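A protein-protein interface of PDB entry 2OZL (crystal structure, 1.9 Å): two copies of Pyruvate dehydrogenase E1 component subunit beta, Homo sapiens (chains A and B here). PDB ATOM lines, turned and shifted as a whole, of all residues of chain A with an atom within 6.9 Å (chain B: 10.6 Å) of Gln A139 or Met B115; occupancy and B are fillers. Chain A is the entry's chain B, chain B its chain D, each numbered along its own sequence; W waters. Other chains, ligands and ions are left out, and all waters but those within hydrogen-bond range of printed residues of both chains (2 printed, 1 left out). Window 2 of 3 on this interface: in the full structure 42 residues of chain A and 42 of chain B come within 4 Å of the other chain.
Among the printed residues, pairs that only touch across the chains: Met A99 with Ile B102, Met A99 with Asp B103, Met A99 with Asn B107, Ala A138 with Met B115, Gln A139 with Met B115, Gln A142 with Ile B106, Pro A313 with Lys B111, Pro A313 with Tyr B114 and Pro A313 with Pro B152.
Printed residues of chain B that touch a printed residue of chain A: Ile B102, Asp B103, Ile B106, Asn B107, Lys B111, Tyr B114, Met B115 and Pro B152.
Hydrophobic or aromatic side chains of chain A that line the printed part of chain B: Met A99, Ala A138 and Pro A313.
Among the printed residues, 12 pairs touch across the chains.
Among the printed residues, no Asp or Glu carboxylate lies within 4 Å of a Lys or Arg side-chain nitrogen of the other chain.
The side-chain amide oxygen (OD1) of Asn A96 sits close to the backbone carbonyl oxygen (O) of Gln A139 (3.5 Å).
The backbone NH (N) of Gln A142 is in hydrogen-bond range of the side-chain amide oxygen (OD1) of Asn A96 (3.0 Å).
The backbone carbonyl oxygen (O) of Met A314 is in hydrogen-bond range of the backbone NH (N) of Ala A138, at 2.9 Å.
OD1 of Asp B103 is in hydrogen-bond range of ND2 of Asn B107, 2.7 Å away.
The backbone NH of Ser B108 sits at hydrogen-bond distance from the backbone carbonyl oxygen of Asp B103 (3.5 Å).
O of Ile B106 lies within hydrogen-bond range of N of Lys B111 (3.3 Å).
Gln A139 touches just these residues of chain B: Asn B107 (2.8 Å) and Met B115 (3.8 Å).
No residue of chain B comes within 4 Å of Asn A96.
Ala A138 touches two residues of chain B.
No residue of chain B comes within 4 Å of His A140.
Printed residues of chain B within 4 Å of Gln A142: Ile B106 (3.7 Å) and Lys B111 (2.9 Å).
Of the printed residues of chain A, Ile B106 touches Gln A142.
Printed residues of chain A within 4 Å of Pro B152: Pro A313.
Printed residues of chain A within 4 Å of Ile B102: Met A99 (3.7 Å).
Ser B108 touches none of the printed residues of chain A.
Ser A141 touches none of the printed residues of chain B.
Water W2 bridges O of Asn A96 (2.9 Å) and OD1 of Asp B103 (3.1 Å).
Water W1 lies within hydrogen-bond range of O of Met A99 (3.0 Å), N of Asp B103 (3.0 Å) and N of Ile B102 (3.3 Å).
O of Ala A138 is in hydrogen-bond range of NZ of Lys B111 (2.9 Å).
NE2 of Gln A139 lies within hydrogen-bond range of O of Asn B107, 2.8 Å away.
NZ of Lys B111 lies within hydrogen-bond range of OE1 of Gln A142, at 2.9 Å.
No position is printed for both chains.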
ATOM      1  N   THR A  94     -15.380 -34.284  12.564  1.00  0.00           N
ATOM      2  CA  THR A  94     -14.487 -33.509  13.429  1.00  0.00           C
ATOM      3  C   THR A  94     -14.239 -34.506  14.551  1.00  0.00           C
ATOM      4  O   THR A  94     -15.050 -35.414  14.754  1.00  0.00           O
ATOM      5  CB  THR A  94     -15.123 -32.215  14.020  1.00  0.00           C
ATOM      6  OG1 THR A  94     -16.154 -32.554  14.953  1.00  0.00           O
ATOM      7  CG2 THR A  94     -15.685 -31.335  12.913  1.00  0.00           C
ATOM      8  N   ASN A  96     -14.503 -34.031  17.595  1.00  0.00           N
ATOM      9  CA  ASN A  96     -15.456 -33.794  18.677  1.00  0.00           C
ATOM     10  C   ASN A  96     -16.477 -34.923  18.612  1.00  0.00           C
ATOM     11  O   ASN A  96     -16.966 -35.395  19.636  1.00  0.00           O
ATOM     12  CB  ASN A  96     -16.198 -32.471  18.480  1.00  0.00           C
ATOM     13  CG  ASN A  96     -15.273 -31.277  18.444  1.00  0.00           C
ATOM     14  OD1 ASN A  96     -14.741 -30.860  19.473  1.00  0.00           O
ATOM     15  ND2 ASN A  96     -15.072 -30.721  17.251  1.00  0.00           N
ATOM     16  N   PHE A  97     -16.788 -35.348  17.389  1.00  0.00           N
ATOM     17  CA  PHE A  97     -17.765 -36.405  17.152  1.00  0.00           C
ATOM     18  C   PHE A  97     -17.200 -37.802  17.392  1.00  0.00           C
ATOM     19  O   PHE A  97     -17.953 -38.773  17.434  1.00  0.00           O
ATOM     20  CB  PHE A  97     -18.299 -36.317  15.717  1.00  0.00           C
ATOM     21  CG  PHE A  97     -18.701 -34.929  15.300  1.00  0.00           C
ATOM     22  CD1 PHE A  97     -18.578 -34.530  13.971  1.00  0.00           C
ATOM     23  CD2 PHE A  97     -19.181 -34.010  16.233  1.00  0.00           C
ATOM     24  CE1 PHE A  97     -18.920 -33.241  13.576  1.00  0.00           C
ATOM     25  CE2 PHE A  97     -19.528 -32.714  15.847  1.00  0.00           C
ATOM     26  CZ  PHE A  97     -19.395 -32.329  14.516  1.00  0.00           C
ATOM     27  N   MET A  99     -16.035 -38.785  20.069  1.00  0.00           N
ATOM     28  CA  MET A  99     -16.340 -39.168  21.442  1.00  0.00           C
ATOM     29  C   MET A  99     -17.437 -40.225  21.498  1.00  0.00           C
ATOM     30  O   MET A  99     -17.426 -41.092  22.369  1.00  0.00           O
ATOM     31  CB  MET A  99     -16.742 -37.950  22.287  1.00  0.00           C
ATOM     32  CG  MET A  99     -15.549 -37.097  22.744  1.00  0.00           C
ATOM     33  SD  MET A  99     -15.931 -35.970  24.127  1.00  0.00           S
ATOM     34  CE  MET A  99     -16.860 -34.715  23.286  1.00  0.00           C
ATOM     35  N   VAL A 136     -16.863 -21.805  15.886  1.00  0.00           N
ATOM     36  CA  VAL A 136     -17.721 -22.983  15.993  1.00  0.00           C
ATOM     37  C   VAL A 136     -18.199 -23.320  17.414  1.00  0.00           C
ATOM     38  O   VAL A 136     -18.911 -24.300  17.614  1.00  0.00           O
ATOM     39  CB  VAL A 136     -17.043 -24.219  15.358  1.00  0.00           C
ATOM     40  CG1 VAL A 136     -16.842 -23.979  13.858  1.00  0.00           C
ATOM     41  CG2 VAL A 136     -15.714 -24.496  16.026  1.00  0.00           C
ATOM     42  N   ALA A 137     -17.806 -22.512  18.395  1.00  0.00           N
ATOM     43  CA  ALA A 137     -18.243 -22.698  19.780  1.00  0.00           C
ATOM     44  C   ALA A 137     -17.731 -23.936  20.530  1.00  0.00           C
ATOM     45  O   ALA A 137     -16.995 -24.765  19.987  1.00  0.00           O
ATOM     46  CB  ALA A 137     -19.781 -22.638  19.847  1.00  0.00           C
ATOM     47  N   ALA A 138     -18.159 -24.047  21.785  1.00  0.00           N
ATOM     48  CA  ALA A 138     -17.727 -25.097  22.713  1.00  0.00           C
ATOM     49  C   ALA A 138     -17.763 -26.574  22.325  1.00  0.00           C
ATOM     50  O   ALA A 138     -16.812 -27.306  22.618  1.00  0.00           O
ATOM     51  CB  ALA A 138     -18.448 -24.907  24.049  1.00  0.00           C
ATOM     52  N   GLN A 139     -18.835 -27.025  21.685  1.00  0.00           N
ATOM     53  CA  GLN A 139     -18.938 -28.434  21.319  1.00  0.00           C
ATOM     54  C   GLN A 139     -18.196 -28.815  20.040  1.00  0.00           C
ATOM     55  O   GLN A 139     -18.112 -29.997  19.703  1.00  0.00           O
ATOM     56  CB  GLN A 139     -20.417 -28.833  21.192  1.00  0.00           C
ATOM     57  CG  GLN A 139     -21.266 -28.480  22.414  1.00  0.00           C
ATOM     58  CD  GLN A 139     -22.700 -28.979  22.312  1.00  0.00           C
ATOM     59  OE1 GLN A 139     -23.343 -28.860  21.264  1.00  0.00           O
ATOM     60  NE2 GLN A 139     -23.215 -29.524  23.409  1.00  0.00           N
ATOM     61  N   HIS A 140     -17.641 -27.829  19.340  1.00  0.00           N
ATOM     62  CA  HIS A 140     -16.941 -28.090  18.083  1.00  0.00           C
ATOM     63  C   HIS A 140     -15.474 -27.670  18.036  1.00  0.00           C
ATOM     64  O   HIS A 140     -14.853 -27.729  16.973  1.00  0.00           O
ATOM     65  CB  HIS A 140     -17.671 -27.388  16.931  1.00  0.00           C
ATOM     66  CG  HIS A 140     -18.964 -28.033  16.542  1.00  0.00           C
ATOM     67  ND1 HIS A 140     -20.066 -28.061  17.370  1.00  0.00           N
ATOM     68  CD2 HIS A 140     -19.333 -28.666  15.403  1.00  0.00           C
ATOM     69  CE1 HIS A 140     -21.057 -28.681  16.757  1.00  0.00           C
ATOM     70  NE2 HIS A 140     -20.639 -29.059  15.561  1.00  0.00           N
ATOM     71  N   SER A 141     -14.912 -27.279  19.176  1.00  0.00           N
ATOM     72  CA  SER A 141     -13.530 -26.795  19.219  1.00  0.00           C
ATOM     73  C   SER A 141     -12.516 -27.611  20.027  1.00  0.00           C
ATOM     74  O   SER A 141     -11.367 -27.191  20.180  1.00  0.00           O
ATOM     75  CB  SER A 141     -13.533 -25.364  19.766  1.00  0.00           C
ATOM     76  OG  SER A 141     -14.447 -24.544  19.052  1.00  0.00           O
ATOM     77  N   GLN A 142     -12.916 -28.773  20.522  1.00  0.00           N
ATOM     78  CA  GLN A 142     -12.033 -29.581  21.361  1.00  0.00           C
ATOM     79  C   GLN A 142     -10.852 -30.281  20.686  1.00  0.00           C
ATOM     80  O   GLN A 142     -10.985 -30.828  19.595  1.00  0.00           O
ATOM     81  CB  GLN A 142     -12.874 -30.619  22.106  1.00  0.00           C
ATOM     82  CG  GLN A 142     -12.262 -31.129  23.396  1.00  0.00           C
ATOM     83  CD  GLN A 142     -13.224 -32.014  24.157  1.00  0.00           C
ATOM     84  OE1 GLN A 142     -14.426 -31.749  24.188  1.00  0.00           O
ATOM     85  NE2 GLN A 142     -12.705 -33.067  24.781  1.00  0.00           N
ATOM     86  N   PRO A 313     -14.392 -23.678  28.164  1.00  0.00           N
ATOM     87  CA  PRO A 313     -14.970 -24.259  26.954  1.00  0.00           C
ATOM     88  C   PRO A 313     -14.908 -23.108  25.950  1.00  0.00           C
ATOM     89  O   PRO A 313     -15.054 -21.946  26.332  1.00  0.00           O
ATOM     90  CB  PRO A 313     -16.395 -24.632  27.376  1.00  0.00           C
ATOM     91  CG  PRO A 313     -16.634 -23.857  28.632  1.00  0.00           C
ATOM     92  CD  PRO A 313     -15.307 -23.801  29.309  1.00  0.00           C
ATOM     93  N   MET A 314     -14.678 -23.419  24.682  1.00  0.00           N
ATOM     94  CA  MET A 314     -14.530 -22.372  23.675  1.00  0.00           C
ATOM     95  C   MET A 314     -15.727 -21.447  23.467  1.00  0.00           C
ATOM     96  O   MET A 314     -16.816 -21.893  23.097  1.00  0.00           O
ATOM     97  CB  MET A 314     -14.128 -22.995  22.330  1.00  0.00           C
ATOM     98  CG  MET A 314     -13.699 -21.981  21.272  1.00  0.00           C
ATOM     99  SD  MET A 314     -12.120 -21.170  21.679  1.00  0.00           S
ATOM    100  CE  MET A 314     -10.949 -22.480  21.206  1.00  0.00           C
ATOM    101  N   VAL B  79     -28.749 -36.201  32.667  1.00  0.00           N
ATOM    102  CA  VAL B  79     -28.397 -34.806  32.417  1.00  0.00           C
ATOM    103  C   VAL B  79     -29.634 -33.952  32.145  1.00  0.00           C
ATOM    104  O   VAL B  79     -29.725 -32.812  32.607  1.00  0.00           O
ATOM    105  CB  VAL B  79     -27.413 -34.672  31.229  1.00  0.00           C
ATOM    106  CG1 VAL B  79     -27.155 -33.199  30.927  1.00  0.00           C
ATOM    107  CG2 VAL B  79     -26.098 -35.366  31.562  1.00  0.00           C
ATOM    108  N   MET B  83     -31.072 -30.633  34.252  1.00  0.00           N
ATOM    109  CA  MET B  83     -31.363 -29.336  33.651  1.00  0.00           C
ATOM    110  C   MET B  83     -32.763 -28.877  34.040  1.00  0.00           C
ATOM    111  O   MET B  83     -33.033 -27.675  34.149  1.00  0.00           O
ATOM    112  CB  MET B  83     -31.274 -29.411  32.127  1.00  0.00           C
ATOM    113  CG  MET B  83     -29.909 -29.783  31.586  1.00  0.00           C
ATOM    114  SD  MET B  83     -29.808 -29.524  29.797  1.00  0.00           S
ATOM    115  CE  MET B  83     -30.836 -30.830  29.208  1.00  0.00           C
ATOM    116  N   ILE B 102     -19.435 -40.722  27.206  1.00  0.00           N
ATOM    117  CA  ILE B 102     -18.584 -39.581  27.493  1.00  0.00           C
ATOM    118  C   ILE B 102     -18.990 -38.270  26.804  1.00  0.00           C
ATOM    119  O   ILE B 102     -18.686 -37.183  27.306  1.00  0.00           O
ATOM    120  CB  ILE B 102     -17.096 -39.943  27.217  1.00  0.00           C
ATOM    121  CG1 ILE B 102     -16.187 -39.046  28.059  1.00  0.00           C
ATOM    122  CG2 ILE B 102     -16.784 -39.808  25.733  1.00  0.00           C
ATOM    123  CD1 ILE B 102     -14.768 -39.563  28.183  1.00  0.00           C
ATOM    124  N   ASP B 103     -19.695 -38.352  25.679  1.00  0.00           N
ATOM    125  CA  ASP B 103     -20.134 -37.125  25.012  1.00  0.00           C
ATOM    126  C   ASP B 103     -21.162 -36.388  25.867  1.00  0.00           C
ATOM    127  O   ASP B 103     -21.151 -35.159  25.926  1.00  0.00           O
ATOM    128  CB  ASP B 103     -20.769 -37.402  23.650  1.00  0.00           C
ATOM    129  CG  ASP B 103     -21.314 -36.129  23.001  1.00  0.00           C
ATOM    130  OD1 ASP B 103     -20.506 -35.336  22.463  1.00  0.00           O
ATOM    131  OD2 ASP B 103     -22.549 -35.910  23.048  1.00  0.00           O
ATOM    132  N   GLN B 104     -22.060 -37.130  26.513  1.00  0.00           N
ATOM    133  CA  GLN B 104     -23.080 -36.502  27.363  1.00  0.00           C
ATOM    134  C   GLN B 104     -22.434 -35.843  28.578  1.00  0.00           C
ATOM    135  O   GLN B 104     -22.877 -34.784  29.027  1.00  0.00           O
ATOM    136  CB  GLN B 104     -24.118 -37.529  27.838  1.00  0.00           C
ATOM    137  CG  GLN B 104     -25.064 -38.049  26.751  1.00  0.00           C
ATOM    138  CD  GLN B 104     -26.110 -37.037  26.307  1.00  0.00           C
ATOM    139  OE1 GLN B 104     -26.089 -35.877  26.718  1.00  0.00           O
ATOM    140  NE2 GLN B 104     -27.034 -37.481  25.457  1.00  0.00           N
ATOM    141  N   VAL B 105     -21.392 -36.472  29.111  1.00  0.00           N
ATOM    142  CA  VAL B 105     -20.702 -35.928  30.274  1.00  0.00           C
ATOM    143  C   VAL B 105     -19.988 -34.634  29.917  1.00  0.00           C
ATOM    144  O   VAL B 105     -20.076 -33.645  30.644  1.00  0.00           O
ATOM    145  CB  VAL B 105     -19.641 -36.910  30.826  1.00  0.00           C
ATOM    146  CG1 VAL B 105     -18.966 -36.311  32.058  1.00  0.00           C
ATOM    147  CG2 VAL B 105     -20.286 -38.244  31.170  1.00  0.00           C
ATOM    148  N   ILE B 106     -19.291 -34.641  28.786  1.00  0.00           N
ATOM    149  CA  ILE B 106     -18.523 -33.479  28.348  1.00  0.00           C
ATOM    150  C   ILE B 106     -19.298 -32.391  27.605  1.00  0.00           C
ATOM    151  O   ILE B 106     -19.329 -31.239  28.043  1.00  0.00           O
ATOM    152  CB  ILE B 106     -17.332 -33.916  27.461  1.00  0.00           C
ATOM    153  CG1 ILE B 106     -16.464 -34.924  28.220  1.00  0.00           C
ATOM    154  CG2 ILE B 106     -16.502 -32.707  27.061  1.00  0.00           C
ATOM    155  CD1 ILE B 106     -15.903 -34.397  29.528  1.00  0.00           C
ATOM    156  N   ASN B 107     -19.923 -32.745  26.488  1.00  0.00           N
ATOM    157  CA  ASN B 107     -20.650 -31.750  25.709  1.00  0.00           C
ATOM    158  C   ASN B 107     -22.026 -31.340  26.233  1.00  0.00           C
ATOM    159  O   ASN B 107     -22.447 -30.201  26.025  1.00  0.00           O
ATOM    160  CB  ASN B 107     -20.767 -32.201  24.249  1.00  0.00           C
ATOM    161  CG  ASN B 107     -19.462 -32.027  23.477  1.00  0.00           C
ATOM    162  OD1 ASN B 107     -18.723 -31.065  23.693  1.00  0.00           O
ATOM    163  ND2 ASN B 107     -19.187 -32.945  22.560  1.00  0.00           N
ATOM    164  N   SER B 108     -22.729 -32.246  26.910  1.00  0.00           N
ATOM    165  CA  SER B 108     -24.050 -31.907  27.432  1.00  0.00           C
ATOM    166  C   SER B 108     -24.047 -31.366  28.860  1.00  0.00           C
ATOM    167  O   SER B 108     -24.796 -30.442  29.176  1.00  0.00           O
ATOM    168  CB  SER B 108     -24.987 -33.116  27.364  1.00  0.00           C
ATOM    169  OG  SER B 108     -25.351 -33.422  26.028  1.00  0.00           O
ATOM    170  N   ALA B 109     -23.213 -31.934  29.725  1.00  0.00           N
ATOM    171  CA  ALA B 109     -23.172 -31.502  31.117  1.00  0.00           C
ATOM    172  C   ALA B 109     -22.120 -30.446  31.446  1.00  0.00           C
ATOM    173  O   ALA B 109     -22.453 -29.355  31.893  1.00  0.00           O
ATOM    174  CB  ALA B 109     -22.978 -32.713  32.027  1.00  0.00           C
ATOM    175  N   ALA B 110     -20.852 -30.767  31.218  1.00  0.00           N
ATOM    176  CA  ALA B 110     -19.764 -29.855  31.554  1.00  0.00           C
ATOM    177  C   ALA B 110     -19.767 -28.468  30.914  1.00  0.00           C
ATOM    178  O   ALA B 110     -19.524 -27.470  31.594  1.00  0.00           O
ATOM    179  CB  ALA B 110     -18.422 -30.534  31.284  1.00  0.00           C
ATOM    180  N   LYS B 111     -20.046 -28.399  29.618  1.00  0.00           N
ATOM    181  CA  LYS B 111     -20.009 -27.126  28.907  1.00  0.00           C
ATOM    182  C   LYS B 111     -21.272 -26.265  28.930  1.00  0.00           C
ATOM    183  O   LYS B 111     -21.209 -25.076  28.622  1.00  0.00           O
ATOM    184  CB  LYS B 111     -19.608 -27.386  27.449  1.00  0.00           C
ATOM    185  CG  LYS B 111     -18.245 -28.063  27.299  1.00  0.00           C
ATOM    186  CD  LYS B 111     -18.006 -28.525  25.870  1.00  0.00           C
ATOM    187  CE  LYS B 111     -16.602 -29.077  25.700  1.00  0.00           C
ATOM    188  NZ  LYS B 111     -16.408 -29.666  24.340  1.00  0.00           N
ATOM    189  N   THR B 112     -22.404 -26.842  29.314  1.00  0.00           N
ATOM    190  CA  THR B 112     -23.669 -26.110  29.285  1.00  0.00           C
ATOM    191  C   THR B 112     -23.819 -24.822  30.090  1.00  0.00           C
ATOM    192  O   THR B 112     -24.330 -23.838  29.558  1.00  0.00           O
ATOM    193  CB  THR B 112     -24.854 -27.058  29.595  1.00  0.00           C
ATOM    194  OG1 THR B 112     -25.002 -27.976  28.505  1.00  0.00           O
ATOM    195  CG2 THR B 112     -26.165 -26.278  29.744  1.00  0.00           C
ATOM    196  N   TYR B 113     -23.391 -24.795  31.347  1.00  0.00           N
ATOM    197  CA  TYR B 113     -23.543 -23.560  32.116  1.00  0.00           C
ATOM    198  C   TYR B 113     -22.817 -22.404  31.423  1.00  0.00           C
ATOM    199  O   TYR B 113     -23.347 -21.295  31.325  1.00  0.00           O
ATOM    200  CB  TYR B 113     -23.007 -23.729  33.544  1.00  0.00           C
ATOM    201  CG  TYR B 113     -23.435 -22.616  34.477  1.00  0.00           C
ATOM    202  CD1 TYR B 113     -22.497 -21.764  35.063  1.00  0.00           C
ATOM    203  CD2 TYR B 113     -24.787 -22.401  34.758  1.00  0.00           C
ATOM    204  CE1 TYR B 113     -22.896 -20.722  35.910  1.00  0.00           C
ATOM    205  CE2 TYR B 113     -25.195 -21.363  35.597  1.00  0.00           C
ATOM    206  CZ  TYR B 113     -24.246 -20.529  36.167  1.00  0.00           C
ATOM    207  OH  TYR B 113     -24.658 -19.501  36.985  1.00  0.00           O
ATOM    208  N   TYR B 114     -21.613 -22.676  30.925  1.00  0.00           N
ATOM    209  CA  TYR B 114     -20.801 -21.669  30.248  1.00  0.00           C
ATOM    210  C   TYR B 114     -21.419 -21.230  28.926  1.00  0.00           C
ATOM    211  O   TYR B 114     -21.491 -20.037  28.636  1.00  0.00           O
ATOM    212  CB  TYR B 114     -19.392 -22.218  29.987  1.00  0.00           C
ATOM    213  CG  TYR B 114     -18.421 -21.210  29.408  1.00  0.00           C
ATOM    214  CD1 TYR B 114     -17.735 -20.311  30.232  1.00  0.00           C
ATOM    215  CD2 TYR B 114     -18.194 -21.147  28.032  1.00  0.00           C
ATOM    216  CE1 TYR B 114     -16.849 -19.381  29.697  1.00  0.00           C
ATOM    217  CE2 TYR B 114     -17.317 -20.226  27.489  1.00  0.00           C
ATOM    218  CZ  TYR B 114     -16.645 -19.344  28.322  1.00  0.00           C
ATOM    219  OH  TYR B 114     -15.773 -18.433  27.767  1.00  0.00           O
ATOM    220  N   MET B 115     -21.859 -22.194  28.119  1.00  0.00           N
ATOM    221  CA  MET B 115     -22.458 -21.874  26.825  1.00  0.00           C
ATOM    222  C   MET B 115     -23.736 -21.057  26.955  1.00  0.00           C
ATOM    223  O   MET B 115     -24.010 -20.188  26.128  1.00  0.00           O
ATOM    224  CB  MET B 115     -22.746 -23.154  26.024  1.00  0.00           C
ATOM    225  CG  MET B 115     -21.488 -23.846  25.491  1.00  0.00           C
ATOM    226  SD  MET B 115     -21.843 -25.203  24.346  1.00  0.00           S
ATOM    227  CE  MET B 115     -22.709 -26.343  25.442  1.00  0.00           C
ATOM    228  N   SER B 116     -24.508 -21.329  28.002  1.00  0.00           N
ATOM    229  CA  SER B 116     -25.770 -20.626  28.232  1.00  0.00           C
ATOM    230  C   SER B 116     -25.571 -19.262  28.879  1.00  0.00           C
ATOM    231  O   SER B 116     -26.540 -18.556  29.156  1.00  0.00           O
ATOM    232  CB  SER B 116     -26.682 -21.460  29.127  1.00  0.00           C
ATOM    233  OG  SER B 116     -26.147 -21.542  30.434  1.00  0.00           O
ATOM    234  N   GLY B 117     -24.320 -18.894  29.131  1.00  0.00           N
ATOM    235  CA  GLY B 117     -24.054 -17.613  29.757  1.00  0.00           C
ATOM    236  C   GLY B 117     -24.546 -17.556  31.191  1.00  0.00           C
ATOM    237  O   GLY B 117     -25.013 -16.516  31.652  1.00  0.00           O
ATOM    238  N   GLY B 118     -24.456 -18.683  31.891  1.00  0.00           N
ATOM    239  CA  GLY B 118     -24.878 -18.744  33.280  1.00  0.00           C
ATOM    240  C   GLY B 118     -26.371 -18.898  33.517  1.00  0.00           C
ATOM    241  O   GLY B 118     -26.872 -18.526  34.577  1.00  0.00           O
ATOM    242  N   LEU B 119     -27.092 -19.448  32.545  1.00  0.00           N
ATOM    243  CA  LEU B 119     -28.533 -19.624  32.703  1.00  0.00           C
ATOM    244  C   LEU B 119     -28.957 -21.067  32.980  1.00  0.00           C
ATOM    245  O   LEU B 119     -29.961 -21.299  33.648  1.00  0.00           O
ATOM    246  CB  LEU B 119     -29.272 -19.108  31.460  1.00  0.00           C
ATOM    247  CG  LEU B 119     -29.459 -17.591  31.308  1.00  0.00           C
ATOM    248  CD1 LEU B 119     -28.137 -16.866  31.503  1.00  0.00           C
ATOM    249  CD2 LEU B 119     -30.032 -17.286  29.931  1.00  0.00           C
ATOM    250  N   GLN B 120     -28.188 -22.034  32.487  1.00  0.00           N
ATOM    251  CA  GLN B 120     -28.549 -23.433  32.677  1.00  0.00           C
ATOM    252  C   GLN B 120     -27.557 -24.266  33.482  1.00  0.00           C
ATOM    253  O   GLN B 120     -26.572 -24.769  32.938  1.00  0.00           O
ATOM    254  CB  GLN B 120     -28.762 -24.102  31.316  1.00  0.00           C
ATOM    255  CG  GLN B 120     -29.246 -25.547  31.411  1.00  0.00           C
ATOM    256  CD  GLN B 120     -30.625 -25.650  32.035  1.00  0.00           C
ATOM    257  OE1 GLN B 120     -31.623 -25.242  31.436  1.00  0.00           O
ATOM    258  NE2 GLN B 120     -30.688 -26.187  33.248  1.00  0.00           N
ATOM    259  N   PRO B 121     -27.799 -24.422  34.791  1.00  0.00           N
ATOM    260  CA  PRO B 121     -26.882 -25.222  35.606  1.00  0.00           C
ATOM    261  C   PRO B 121     -27.204 -26.707  35.427  1.00  0.00           C
ATOM    262  O   PRO B 121     -28.296 -27.059  34.961  1.00  0.00           O
ATOM    263  CB  PRO B 121     -27.165 -24.728  37.018  1.00  0.00           C
ATOM    264  CG  PRO B 121     -28.633 -24.448  36.965  1.00  0.00           C
ATOM    265  CD  PRO B 121     -28.783 -23.727  35.642  1.00  0.00           C
ATOM    266  N   VAL B 122     -26.258 -27.570  35.794  1.00  0.00           N
ATOM    267  CA  VAL B 122     -26.444 -29.010  35.656  1.00  0.00           C
ATOM    268  C   VAL B 122     -25.989 -29.735  36.924  1.00  0.00           C
ATOM    269  O   VAL B 122     -24.857 -30.216  37.003  1.00  0.00           O
ATOM    270  CB  VAL B 122     -25.631 -29.565  34.458  1.00  0.00           C
ATOM    271  CG1 VAL B 122     -26.030 -31.017  34.178  1.00  0.00           C
ATOM    272  CG2 VAL B 122     -25.842 -28.689  33.227  1.00  0.00           C
ATOM    273  N   PRO B 152     -12.750 -28.538  31.265  1.00  0.00           N
ATOM    274  CA  PRO B 152     -13.320 -27.362  31.938  1.00  0.00           C
ATOM    275  C   PRO B 152     -14.830 -27.520  32.138  1.00  0.00           C
ATOM    276  O   PRO B 152     -15.523 -28.070  31.276  1.00  0.00           O
ATOM    277  CB  PRO B 152     -13.009 -26.218  30.969  1.00  0.00           C
ATOM    278  CG  PRO B 152     -11.741 -26.664  30.307  1.00  0.00           C
ATOM    279  CD  PRO B 152     -12.011 -28.136  30.053  1.00  0.00           C
ATOM    280  N   GLY B 153     -15.335 -27.037  33.271  1.00  0.00           N
ATOM    281  CA  GLY B 153     -16.759 -27.122  33.547  1.00  0.00           C
ATOM    282  C   GLY B 153     -17.120 -28.343  34.368  1.00  0.00           C
ATOM    283  O   GLY B 153     -18.246 -28.498  34.834  1.00  0.00           O
ATOM    284  N   ASN B 177     -23.043 -28.323  39.967  1.00  0.00           N
ATOM    285  CA  ASN B 177     -22.377 -28.539  38.682  1.00  0.00           C
ATOM    286  C   ASN B 177     -22.038 -30.009  38.483  1.00  0.00           C
ATOM    287  O   ASN B 177     -22.098 -30.784  39.415  1.00  0.00           O
ATOM    288  CB  ASN B 177     -21.097 -27.713  38.650  1.00  0.00           C
ATOM    289  CG  ASN B 177     -21.355 -26.255  38.931  1.00  0.00           C
ATOM    290  OD1 ASN B 177     -21.897 -25.544  38.092  1.00  0.00           O
ATOM    291  ND2 ASN B 177     -20.989 -25.804  40.130  1.00  0.00           N
HETATM  292  O   HOH W   1     -19.932 -40.739  23.897  1.00  0.00           O
HETATM  293  O   HOH W   2     -19.282 -36.991  20.177  1.00  0.00           O
